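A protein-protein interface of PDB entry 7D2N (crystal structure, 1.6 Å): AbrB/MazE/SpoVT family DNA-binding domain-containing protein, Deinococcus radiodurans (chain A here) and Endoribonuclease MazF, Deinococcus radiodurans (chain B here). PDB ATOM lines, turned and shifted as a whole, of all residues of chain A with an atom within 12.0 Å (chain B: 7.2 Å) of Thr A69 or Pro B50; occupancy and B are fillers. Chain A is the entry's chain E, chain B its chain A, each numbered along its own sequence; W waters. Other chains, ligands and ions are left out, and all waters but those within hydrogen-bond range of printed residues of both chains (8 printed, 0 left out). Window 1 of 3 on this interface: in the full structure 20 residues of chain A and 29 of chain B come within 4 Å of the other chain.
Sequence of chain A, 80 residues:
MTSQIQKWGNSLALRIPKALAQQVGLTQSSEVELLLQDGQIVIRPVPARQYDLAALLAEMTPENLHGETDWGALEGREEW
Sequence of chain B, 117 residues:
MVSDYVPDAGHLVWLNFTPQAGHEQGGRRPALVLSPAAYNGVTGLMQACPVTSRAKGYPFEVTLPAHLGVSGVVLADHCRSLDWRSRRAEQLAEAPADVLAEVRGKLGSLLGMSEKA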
ATOM      1  N   ASN A  64       3.690 -15.220  20.258  1.00  0.00           N
ATOM      2  CA  ASN A  64       2.580 -15.712  19.452  1.00  0.00           C
ATOM      3  C   ASN A  64       1.371 -14.781  19.446  1.00  0.00           C
ATOM      4  O   ASN A  64       0.392 -15.079  18.760  1.00  0.00           O
ATOM      5  CB  ASN A  64       2.187 -17.154  19.863  1.00  0.00           C
ATOM      6  CG  ASN A  64       1.535 -17.271  21.239  1.00  0.00           C
ATOM      7  OD1 ASN A  64       0.970 -16.330  21.781  1.00  0.00           O
ATOM      8  ND2 ASN A  64       1.579 -18.480  21.789  1.00  0.00           N
ATOM      9  N   LEU A  65       1.437 -13.639  20.127  1.00  0.00           N
ATOM     10  CA  LEU A  65       0.350 -12.664  20.070  1.00  0.00           C
ATOM     11  C   LEU A  65       0.131 -12.146  18.655  1.00  0.00           C
ATOM     12  O   LEU A  65       1.083 -11.891  17.915  1.00  0.00           O
ATOM     13  CB  LEU A  65       0.648 -11.467  20.973  1.00  0.00           C
ATOM     14  CG  LEU A  65       0.817 -11.688  22.467  1.00  0.00           C
ATOM     15  CD1 LEU A  65       0.804 -10.345  23.176  1.00  0.00           C
ATOM     16  CD2 LEU A  65      -0.283 -12.552  22.943  1.00  0.00           C
ATOM     17  N   HIS A  66      -1.134 -11.943  18.293  1.00  0.00           N
ATOM     18  CA  HIS A  66      -1.497 -11.259  17.060  1.00  0.00           C
ATOM     19  C   HIS A  66      -1.987  -9.857  17.375  1.00  0.00           C
ATOM     20  O   HIS A  66      -2.729  -9.659  18.339  1.00  0.00           O
ATOM     21  CB  HIS A  66      -2.593 -12.016  16.301  1.00  0.00           C
ATOM     22  CG  HIS A  66      -2.180 -13.376  15.840  1.00  0.00           C
ATOM     23  ND1 HIS A  66      -1.826 -13.641  14.536  1.00  0.00           N
ATOM     24  CD2 HIS A  66      -2.079 -14.551  16.507  1.00  0.00           C
ATOM     25  CE1 HIS A  66      -1.520 -14.921  14.420  1.00  0.00           C
ATOM     26  NE2 HIS A  66      -1.662 -15.496  15.602  1.00  0.00           N
ATOM     27  N   GLY A  67      -1.587  -8.887  16.552  1.00  0.00           N
ATOM     28  CA  GLY A  67      -2.141  -7.554  16.670  1.00  0.00           C
ATOM     29  C   GLY A  67      -3.561  -7.499  16.125  1.00  0.00           C
ATOM     30  O   GLY A  67      -4.036  -8.411  15.454  1.00  0.00           O
ATOM     31  N   GLU A  68      -4.244  -6.398  16.424  1.00  0.00           N
ATOM     32  CA  GLU A  68      -5.591  -6.165  15.905  1.00  0.00           C
ATOM     33  C   GLU A  68      -5.647  -6.402  14.399  1.00  0.00           C
ATOM     34  O   GLU A  68      -4.780  -5.944  13.654  1.00  0.00           O
ATOM     35  CB  GLU A  68      -6.018  -4.732  16.233  1.00  0.00           C
ATOM     36  CG  GLU A  68      -7.450  -4.389  15.885  1.00  0.00           C
ATOM     37  CD  GLU A  68      -7.736  -2.903  16.044  1.00  0.00           C
ATOM     38  OE1 GLU A  68      -7.223  -2.114  15.219  1.00  0.00           O
ATOM     39  OE2 GLU A  68      -8.457  -2.518  16.992  1.00  0.00           O
ATOM     40  N   THR A  69      -6.668  -7.134  13.954  1.00  0.00           N
ATOM     41  CA  THR A  69      -6.844  -7.362  12.526  1.00  0.00           C
ATOM     42  C   THR A  69      -7.384  -6.103  11.858  1.00  0.00           C
ATOM     43  O   THR A  69      -8.372  -5.514  12.316  1.00  0.00           O
ATOM     44  CB  THR A  69      -7.795  -8.534  12.278  1.00  0.00           C
ATOM     45  OG1 THR A  69      -7.186  -9.746  12.736  1.00  0.00           O
ATOM     46  CG2 THR A  69      -8.094  -8.664  10.760  1.00  0.00           C
ATOM     47  N   ASP A  70      -6.730  -5.693  10.773  1.00  0.00           N
ATOM     48  CA  ASP A  70      -7.108  -4.485  10.054  1.00  0.00           C
ATOM     49  C   ASP A  70      -8.224  -4.795   9.063  1.00  0.00           C
ATOM     50  O   ASP A  70      -8.025  -5.551   8.107  1.00  0.00           O
ATOM     51  CB  ASP A  70      -5.894  -3.900   9.330  1.00  0.00           C
ATOM     52  CG  ASP A  70      -6.243  -2.653   8.525  1.00  0.00           C
ATOM     53  OD1 ASP A  70      -7.159  -1.917   8.945  1.00  0.00           O
ATOM     54  OD2 ASP A  70      -5.591  -2.403   7.484  1.00  0.00           O
ATOM     55  N   TRP A  71      -9.398  -4.208   9.286  1.00  0.00           N
ATOM     56  CA  TRP A  71     -10.478  -4.255   8.307  1.00  0.00           C
ATOM     57  C   TRP A  71     -10.696  -2.884   7.665  1.00  0.00           C
ATOM     58  O   TRP A  71     -11.768  -2.610   7.125  1.00  0.00           O
ATOM     59  CB  TRP A  71     -11.764  -4.791   8.950  1.00  0.00           C
ATOM     60  CG  TRP A  71     -11.741  -6.286   9.185  1.00  0.00           C
ATOM     61  CD1 TRP A  71     -11.615  -6.935  10.390  1.00  0.00           C
ATOM     62  CD2 TRP A  71     -11.839  -7.314   8.188  1.00  0.00           C
ATOM     63  NE1 TRP A  71     -11.629  -8.298  10.195  1.00  0.00           N
ATOM     64  CE2 TRP A  71     -11.774  -8.557   8.858  1.00  0.00           C
ATOM     65  CE3 TRP A  71     -11.994  -7.304   6.794  1.00  0.00           C
ATOM     66  CZ2 TRP A  71     -11.848  -9.772   8.185  1.00  0.00           C
ATOM     67  CZ3 TRP A  71     -12.061  -8.512   6.127  1.00  0.00           C
ATOM     68  CH2 TRP A  71     -11.989  -9.733   6.822  1.00  0.00           C
ATOM     69  N   GLY A  72      -9.677  -2.027   7.693  1.00  0.00           N
ATOM     70  CA  GLY A  72      -9.785  -0.762   6.986  1.00  0.00           C
ATOM     71  C   GLY A  72     -10.861   0.152   7.549  1.00  0.00           C
ATOM     72  O   GLY A  72     -11.192   0.128   8.738  1.00  0.00           O
ATOM     73  N   ALA A  73     -11.413   0.972   6.659  1.00  0.00           N
ATOM     74  CA  ALA A  73     -12.432   1.949   7.007  1.00  0.00           C
ATOM     75  C   ALA A  73     -13.749   1.281   7.385  1.00  0.00           C
ATOM     76  O   ALA A  73     -14.070   0.183   6.927  1.00  0.00           O
ATOM     77  CB  ALA A  73     -12.685   2.883   5.830  1.00  0.00           C
ATOM     78  N   LEU A  74     -14.533   1.996   8.195  1.00  0.00           N
ATOM     79  CA  LEU A  74     -15.903   1.587   8.507  1.00  0.00           C
ATOM     80  C   LEU A  74     -16.725   1.472   7.229  1.00  0.00           C
ATOM     81  O   LEU A  74     -16.664   2.344   6.354  1.00  0.00           O
ATOM     82  CB  LEU A  74     -16.542   2.606   9.457  1.00  0.00           C
ATOM     83  CG  LEU A  74     -17.922   2.312  10.046  1.00  0.00           C
ATOM     84  CD1 LEU A  74     -17.995   2.894  11.450  1.00  0.00           C
ATOM     85  CD2 LEU A  74     -19.032   2.876   9.184  1.00  0.00           C
ATOM     86  N   GLU A  75     -17.505   0.391   7.117  1.00  0.00           N
ATOM     87  CA  GLU A  75     -18.302   0.115   5.927  1.00  0.00           C
ATOM     88  C   GLU A  75     -19.775  -0.055   6.269  1.00  0.00           C
ATOM     89  O   GLU A  75     -20.118  -0.680   7.276  1.00  0.00           O
ATOM     90  CB  GLU A  75     -17.825  -1.159   5.211  1.00  0.00           C
ATOM     91  CG  GLU A  75     -16.405  -1.093   4.725  1.00  0.00           C
ATOM     92  CD  GLU A  75     -16.271  -0.283   3.451  1.00  0.00           C
ATOM     93  OE1 GLU A  75     -17.287   0.281   2.992  1.00  0.00           O
ATOM     94  OE2 GLU A  75     -15.149  -0.214   2.903  1.00  0.00           O
ATOM     95  N   GLU A  78     -21.978  -0.831   9.682  1.00  0.00           N
ATOM     96  CA  GLU A  78     -21.136  -1.028  10.856  1.00  0.00           C
ATOM     97  C   GLU A  78     -21.250   0.156  11.806  1.00  0.00           C
ATOM     98  O   GLU A  78     -21.200   1.314  11.384  1.00  0.00           O
ATOM     99  CB  GLU A  78     -19.679  -1.238  10.433  1.00  0.00           C
ATOM    100  CG  GLU A  78     -19.466  -2.590   9.749  1.00  0.00           C
ATOM    101  CD  GLU A  78     -18.224  -2.669   8.846  1.00  0.00           C
ATOM    102  OE1 GLU A  78     -18.163  -3.631   8.056  1.00  0.00           O
ATOM    103  OE2 GLU A  78     -17.305  -1.817   8.943  1.00  0.00           O
ATOM    104  N   TRP A  80     -19.068   0.640  14.277  1.00  0.00           N
ATOM    105  CA  TRP A  80     -17.695   1.000  14.604  1.00  0.00           C
ATOM    106  C   TRP A  80     -16.747  -0.055  14.036  1.00  0.00           C
ATOM    107  O   TRP A  80     -17.203  -0.948  13.312  1.00  0.00           O
ATOM    108  CB  TRP A  80     -17.517   1.127  16.115  1.00  0.00           C
ATOM    109  CG  TRP A  80     -17.784  -0.128  16.913  1.00  0.00           C
ATOM    110  CD1 TRP A  80     -18.380  -1.296  16.487  1.00  0.00           C
ATOM    111  CD2 TRP A  80     -17.469  -0.318  18.292  1.00  0.00           C
ATOM    112  NE1 TRP A  80     -18.442  -2.198  17.531  1.00  0.00           N
ATOM    113  CE2 TRP A  80     -17.886  -1.622  18.647  1.00  0.00           C
ATOM    114  CE3 TRP A  80     -16.865   0.488  19.266  1.00  0.00           C
ATOM    115  CZ2 TRP A  80     -17.726  -2.128  19.931  1.00  0.00           C
ATOM    116  CZ3 TRP A  80     -16.707  -0.017  20.538  1.00  0.00           C
ATOM    117  CH2 TRP A  80     -17.128  -1.318  20.860  1.00  0.00           C
ATOM    118  N   ARG B  29      -9.652 -10.535   2.268  1.00  0.00           N
ATOM    119  CA  ARG B  29      -9.157 -11.526   3.203  1.00  0.00           C
ATOM    120  C   ARG B  29     -10.269 -12.534   3.451  1.00  0.00           C
ATOM    121  O   ARG B  29     -11.452 -12.157   3.469  1.00  0.00           O
ATOM    122  CB  ARG B  29      -8.740 -10.851   4.517  1.00  0.00           C
ATOM    123  CG  ARG B  29      -8.322 -11.764   5.631  1.00  0.00           C
ATOM    124  CD  ARG B  29      -8.349 -10.984   6.934  1.00  0.00           C
ATOM    125  NE  ARG B  29      -7.311  -9.951   6.985  1.00  0.00           N
ATOM    126  CZ  ARG B  29      -7.537  -8.651   7.167  1.00  0.00           C
ATOM    127  NH1 ARG B  29      -8.774  -8.190   7.298  1.00  0.00           N
ATOM    128  NH2 ARG B  29      -6.506  -7.808   7.220  1.00  0.00           N
ATOM    129  N   PRO B  30      -9.941 -13.814   3.618  1.00  0.00           N
ATOM    130  CA  PRO B  30     -10.983 -14.779   3.982  1.00  0.00           C
ATOM    131  C   PRO B  30     -11.411 -14.606   5.428  1.00  0.00           C
ATOM    132  O   PRO B  30     -10.660 -14.124   6.279  1.00  0.00           O
ATOM    133  CB  PRO B  30     -10.309 -16.144   3.763  1.00  0.00           C
ATOM    134  CG  PRO B  30      -9.062 -15.858   2.977  1.00  0.00           C
ATOM    135  CD  PRO B  30      -8.646 -14.470   3.388  1.00  0.00           C
ATOM    136  N   ALA B  31     -12.650 -15.013   5.697  1.00  0.00           N
ATOM    137  CA  ALA B  31     -13.224 -14.927   7.030  1.00  0.00           C
ATOM    138  C   ALA B  31     -14.208 -16.071   7.213  1.00  0.00           C
ATOM    139  O   ALA B  31     -14.859 -16.507   6.262  1.00  0.00           O
ATOM    140  CB  ALA B  31     -13.934 -13.584   7.253  1.00  0.00           C
ATOM    141  N   LEU B  32     -14.312 -16.557   8.448  1.00  0.00           N
ATOM    142  CA  LEU B  32     -15.271 -17.600   8.794  1.00  0.00           C
ATOM    143  C   LEU B  32     -16.503 -16.959   9.427  1.00  0.00           C
ATOM    144  O   LEU B  32     -16.387 -16.245  10.427  1.00  0.00           O
ATOM    145  CB  LEU B  32     -14.647 -18.607   9.759  1.00  0.00           C
ATOM    146  CG  LEU B  32     -15.638 -19.639  10.290  1.00  0.00           C
ATOM    147  CD1 LEU B  32     -15.999 -20.631   9.193  1.00  0.00           C
ATOM    148  CD2 LEU B  32     -15.031 -20.342  11.488  1.00  0.00           C
ATOM    149  N   ALA B  48     -18.022 -12.478  12.083  1.00  0.00           N
ATOM    150  CA  ALA B  48     -17.078 -13.331  11.379  1.00  0.00           C
ATOM    151  C   ALA B  48     -15.687 -13.193  11.976  1.00  0.00           C
ATOM    152  O   ALA B  48     -15.322 -12.151  12.524  1.00  0.00           O
ATOM    153  CB  ALA B  48     -17.036 -13.011   9.879  1.00  0.00           C
ATOM    154  N   CYS B  49     -14.912 -14.265  11.852  1.00  0.00           N
ATOM    155  CA  CYS B  49     -13.539 -14.307  12.333  1.00  0.00           C
ATOM    156  C   CYS B  49     -12.570 -14.307  11.161  1.00  0.00           C
ATOM    157  O   CYS B  49     -12.770 -15.049  10.190  1.00  0.00           O
ATOM    158  CB  CYS B  49     -13.273 -15.565  13.171  1.00  0.00           C
ATOM    159  SG  CYS B  49     -14.261 -15.708  14.672  1.00  0.00           S
ATOM    160  N   PRO B  50     -11.491 -13.538  11.239  1.00  0.00           N
ATOM    161  CA  PRO B  50     -10.568 -13.456  10.111  1.00  0.00           C
ATOM    162  C   PRO B  50      -9.688 -14.685  10.015  1.00  0.00           C
ATOM    163  O   PRO B  50      -9.358 -15.324  11.019  1.00  0.00           O
ATOM    164  CB  PRO B  50      -9.727 -12.220  10.436  1.00  0.00           C
ATOM    165  CG  PRO B  50      -9.693 -12.223  11.958  1.00  0.00           C
ATOM    166  CD  PRO B  50     -11.069 -12.699  12.377  1.00  0.00           C
ATOM    167  N   VAL B  51      -9.299 -14.996   8.778  1.00  0.00           N
ATOM    168  CA  VAL B  51      -8.268 -15.990   8.493  1.00  0.00           C
ATOM    169  C   VAL B  51      -6.970 -15.234   8.272  1.00  0.00           C
ATOM    170  O   VAL B  51      -6.931 -14.278   7.486  1.00  0.00           O
ATOM    171  CB  VAL B  51      -8.624 -16.830   7.255  1.00  0.00           C
ATOM    172  CG1 VAL B  51      -7.459 -17.767   6.893  1.00  0.00           C
ATOM    173  CG2 VAL B  51      -9.909 -17.597   7.484  1.00  0.00           C
ATOM    174  N   THR B  52      -5.920 -15.631   8.983  1.00  0.00           N
ATOM    175  CA  THR B  52      -4.612 -15.008   8.843  1.00  0.00           C
ATOM    176  C   THR B  52      -3.612 -16.025   8.296  1.00  0.00           C
ATOM    177  O   THR B  52      -3.739 -17.229   8.523  1.00  0.00           O
ATOM    178  CB  THR B  52      -4.135 -14.424  10.199  1.00  0.00           C
ATOM    179  OG1 THR B  52      -2.852 -13.795  10.049  1.00  0.00           O
ATOM    180  CG2 THR B  52      -4.035 -15.502  11.250  1.00  0.00           C
ATOM    181  N   VAL B  73      -5.014 -19.755   9.226  1.00  0.00           N
ATOM    182  CA  VAL B  73      -5.726 -20.194  10.421  1.00  0.00           C
ATOM    183  C   VAL B  73      -6.766 -19.139  10.776  1.00  0.00           C
ATOM    184  O   VAL B  73      -6.597 -17.954  10.470  1.00  0.00           O
ATOM    185  CB  VAL B  73      -4.758 -20.438  11.607  1.00  0.00           C
ATOM    186  CG1 VAL B  73      -3.783 -21.581  11.271  1.00  0.00           C
ATOM    187  CG2 VAL B  73      -3.981 -19.167  11.967  1.00  0.00           C
ATOM    188  N   VAL B  74      -7.836 -19.568  11.452  1.00  0.00           N
ATOM    189  CA  VAL B  74      -8.878 -18.651  11.919  1.00  0.00           C
ATOM    190  C   VAL B  74      -8.477 -18.101  13.283  1.00  0.00           C
ATOM    191  O   VAL B  74      -8.078 -18.865  14.166  1.00  0.00           O
ATOM    192  CB  VAL B  74     -10.243 -19.360  12.003  1.00  0.00           C
ATOM    193  CG1 VAL B  74     -11.322 -18.406  12.537  1.00  0.00           C
ATOM    194  CG2 VAL B  74     -10.652 -19.950  10.642  1.00  0.00           C
ATOM    195  N   LEU B  75      -8.595 -16.781  13.469  1.00  0.00           N
ATOM    196  CA  LEU B  75      -8.369 -16.159  14.781  1.00  0.00           C
ATOM    197  C   LEU B  75      -9.705 -16.049  15.513  1.00  0.00           C
ATOM    198  O   LEU B  75     -10.479 -15.112  15.293  1.00  0.00           O
ATOM    199  CB  LEU B  75      -7.704 -14.797  14.633  1.00  0.00           C
ATOM    200  CG  LEU B  75      -6.278 -14.830  14.088  1.00  0.00           C
ATOM    201  CD1 LEU B  75      -5.714 -13.414  13.999  1.00  0.00           C
ATOM    202  CD2 LEU B  75      -5.397 -15.707  14.965  1.00  0.00           C
ATOM    203  N   ALA B  76      -9.973 -17.008  16.400  1.00  0.00           N
ATOM    204  CA  ALA B  76     -11.295 -17.087  17.015  1.00  0.00           C
ATOM    205  C   ALA B  76     -11.587 -15.862  17.871  1.00  0.00           C
ATOM    206  O   ALA B  76     -12.742 -15.428  17.954  1.00  0.00           O
ATOM    207  CB  ALA B  76     -11.419 -18.354  17.860  1.00  0.00           C
ATOM    208  N   ASP B  77     -10.569 -15.302  18.523  1.00  0.00           N
ATOM    209  CA  ASP B  77     -10.804 -14.158  19.393  1.00  0.00           C
ATOM    210  C   ASP B  77     -10.911 -12.839  18.635  1.00  0.00           C
ATOM    211  O   ASP B  77     -11.159 -11.802  19.265  1.00  0.00           O
ATOM    212  CB  ASP B  77      -9.703 -14.054  20.465  1.00  0.00           C
ATOM    213  CG  ASP B  77      -8.296 -13.890  19.883  1.00  0.00           C
ATOM    214  OD1 ASP B  77      -7.975 -14.490  18.839  1.00  0.00           O
ATOM    215  OD2 ASP B  77      -7.481 -13.178  20.520  1.00  0.00           O
ATOM    216  N   HIS B  78     -10.742 -12.839  17.309  1.00  0.00           N
ATOM    217  CA  HIS B  78     -10.824 -11.616  16.516  1.00  0.00           C
ATOM    218  C   HIS B  78     -12.182 -11.462  15.849  1.00  0.00           C
ATOM    219  O   HIS B  78     -12.315 -10.686  14.899  1.00  0.00           O
ATOM    220  CB  HIS B  78      -9.712 -11.569  15.468  1.00  0.00           C
ATOM    221  CG  HIS B  78      -8.359 -11.284  16.033  1.00  0.00           C
ATOM    222  ND1 HIS B  78      -7.506 -10.364  15.467  1.00  0.00           N
ATOM    223  CD2 HIS B  78      -7.714 -11.787  17.112  1.00  0.00           C
ATOM    224  CE1 HIS B  78      -6.393 -10.311  16.172  1.00  0.00           C
ATOM    225  NE2 HIS B  78      -6.488 -11.168  17.171  1.00  0.00           N
ATOM    226  N   CYS B  79     -13.195 -12.173  16.341  1.00  0.00           N
ATOM    227  CA  CYS B  79     -14.536 -12.054  15.783  1.00  0.00           C
ATOM    228  C   CYS B  79     -15.031 -10.605  15.819  1.00  0.00           C
ATOM    229  O   CYS B  79     -14.758  -9.857  16.763  1.00  0.00           O
ATOM    230  CB  CYS B  79     -15.475 -12.968  16.578  1.00  0.00           C
ATOM    231  SG  CYS B  79     -17.045 -13.281  15.757  1.00  0.00           S
ATOM    232  N   ARG B  80     -15.769 -10.212  14.777  1.00  0.00           N
ATOM    233  CA  ARG B  80     -16.139  -8.813  14.588  1.00  0.00           C
ATOM    234  C   ARG B  80     -17.407  -8.733  13.750  1.00  0.00           C
ATOM    235  O   ARG B  80     -17.588  -9.541  12.848  1.00  0.00           O
ATOM    236  CB  ARG B  80     -14.996  -8.048  13.893  1.00  0.00           C
ATOM    237  CG  ARG B  80     -15.242  -6.587  13.581  1.00  0.00           C
ATOM    238  CD  ARG B  80     -13.916  -5.904  13.328  1.00  0.00           C
ATOM    239  NE  ARG B  80     -14.072  -4.616  12.663  1.00  0.00           N
ATOM    240  CZ  ARG B  80     -13.047  -3.838  12.328  1.00  0.00           C
ATOM    241  NH1 ARG B  80     -11.803  -4.227  12.615  1.00  0.00           N
ATOM    242  NH2 ARG B  80     -13.262  -2.683  11.715  1.00  0.00           N
ATOM    243  N   LEU B  82     -19.328  -7.200  10.807  1.00  0.00           N
ATOM    244  CA  LEU B  82     -18.913  -6.606   9.540  1.00  0.00           C
ATOM    245  C   LEU B  82     -20.081  -6.580   8.566  1.00  0.00           C
ATOM    246  O   LEU B  82     -20.909  -7.491   8.549  1.00  0.00           O
ATOM    247  CB  LEU B  82     -17.740  -7.388   8.920  1.00  0.00           C
ATOM    248  CG  LEU B  82     -16.480  -7.404   9.789  1.00  0.00           C
ATOM    249  CD1 LEU B  82     -15.504  -8.457   9.280  1.00  0.00           C
ATOM    250  CD2 LEU B  82     -15.842  -6.030   9.807  1.00  0.00           C
HETATM  251  O   HOH W   1     -16.633  -3.587  13.117  1.00  0.00           O
HETATM  252  O   HOH W   2     -13.258   0.201  10.879  1.00  0.00           O
HETATM  253  O   HOH W   3     -15.638  -1.129  11.038  1.00  0.00           O
HETATM  254  O   HOH W   4      -8.921  -7.724  16.032  1.00  0.00           O
HETATM  255  O   HOH W   5     -10.409  -1.971  10.809  1.00  0.00           O
HETATM  256  O   HOH W   6     -10.406  -6.515  13.887  1.00  0.00           O
HETATM  257  O   HOH W   7     -11.225  -9.098  13.056  1.00  0.00           O
HETATM  258  O   HOH W   8      -4.369 -11.669  19.117  1.00  0.00           O
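ND1 of His B78 lies within hydrogen-bond range of OG1 of Thr A69 (2.8 Å). NH1 of Arg B29 lies within hydrogen-bond range of O of Asp A70 (2.9 Å).
The side-chain carboxylate (OD1) of Asp A70 sits at hydrogen-bond distance from the backbone NH (N) of Gly A72 (2.8 Å). The backbone NH of Leu B75 sits at hydrogen-bond distance from the backbone carbonyl oxygen of Pro B50 (3.0 Å). The side-chain carboxylate of Glu A78 sits at hydrogen-bond distance from the backbone NH of Glu A75 (2.9 Å). The backbone NH (N) of Arg B80 sits at hydrogen-bond distance from the backbone carbonyl oxygen (O) of Ala B48 (3.0 Å).
Among the printed residues, pairs that only touch across the chains: Gly A67 with His B78 (3.1 Å), Trp A71 with Arg B29 (3.3 Å), Glu A78 with Leu B82 (3.4 Å), Trp A71 with Arg B80 (3.5 Å), Thr A69 with Arg B29 (3.6 Å), Thr A69 with Pro B50 (3.6 Å), Thr A69 with Arg B80 (3.7 Å), Trp A71 with Leu B82 (3.8 Å), His A66 with Leu B75 (3.8 Å) and Trp A71 with Pro B50 (3.9 Å).
Thr A69 touches four residues of chain B. Pro B50 touches just these residues of chain A: Thr A69 and Trp A71. No residue of chain A comes within 4 Å of Pro B30. No residue of chain A comes within 4 Å of Ala B31. No residue of chain A comes within 4 Å of Ala B48. No residue of chain A comes within 4 Å of Val B51. No residue of chain A comes within 4 Å of Thr B52. No residue of chain A comes within 4 Å of Val B74. Of the printed residues of chain A, His B78 touches Gly A67 and Thr A69. Arg B80 touches two residues of chain A. Of the printed residues of chain A, Arg B29 touches Thr A69, Asp A70 and Trp A71. Of the printed residues of chain B, Trp A71 touches Arg B29, Pro B50, Arg B80 and Leu B82. Of the printed residues of chain B, Asp A70 touches Arg B29. The nearest residue of chain B that does not touch Thr A69 is Leu B75 (4.1 Å). The nearest residue of chain A that does not touch Pro B50 is Asp A70 (7.2 Å).
Of the 18 printed residues of chain B, 6 touch a printed residue of chain A. Hydrophobic or aromatic side chains of chain B that line the printed part of chain A: Pro B50, Leu B75, His B78 and Leu B82. Hydrophobic or aromatic side chains of chain A that line the printed part of chain B: His A66 and Trp A71. Along chain A the printed residues that touch a printed residue of chain B span positions 66 to 78. Among the printed residues, 12 pairs touch across the chains. Among the printed residues, no Asp or Glu carboxylate lies within 4 Å of a Lys or Arg side-chain nitrogen of the other chain.
Water W7 lies within hydrogen-bond range of the backbone carbonyl oxygen of His B78 (2.7 Å) and the indole nitrogen of Trp A71 (3.0 Å). Water W6 lies within hydrogen-bond range of the backbone carbonyl oxygen of Thr A69 (2.8 Å) and the guanidinium group of Arg B80 (3.0 Å). Water W3 lies within hydrogen-bond range of OE2 of Glu A78, O of Trp A80 and NH2 of Arg B80. Water W5 lies within hydrogen-bond range of the backbone NH (N) of Trp A71 (2.9 Å), the backbone carbonyl oxygen (O) of Gly A72 (3.1 Å) and the guanidinium group (NH2) of Arg B80 (3.1 Å). Water W2 lies within hydrogen-bond range of the backbone carbonyl oxygen (O) of Gly A72, the guanidinium group (NH2) of Arg B80 and the backbone NH (N) of Leu A74. Water W4 lies within hydrogen-bond range of ND1 of His B78 and N of Thr A69.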
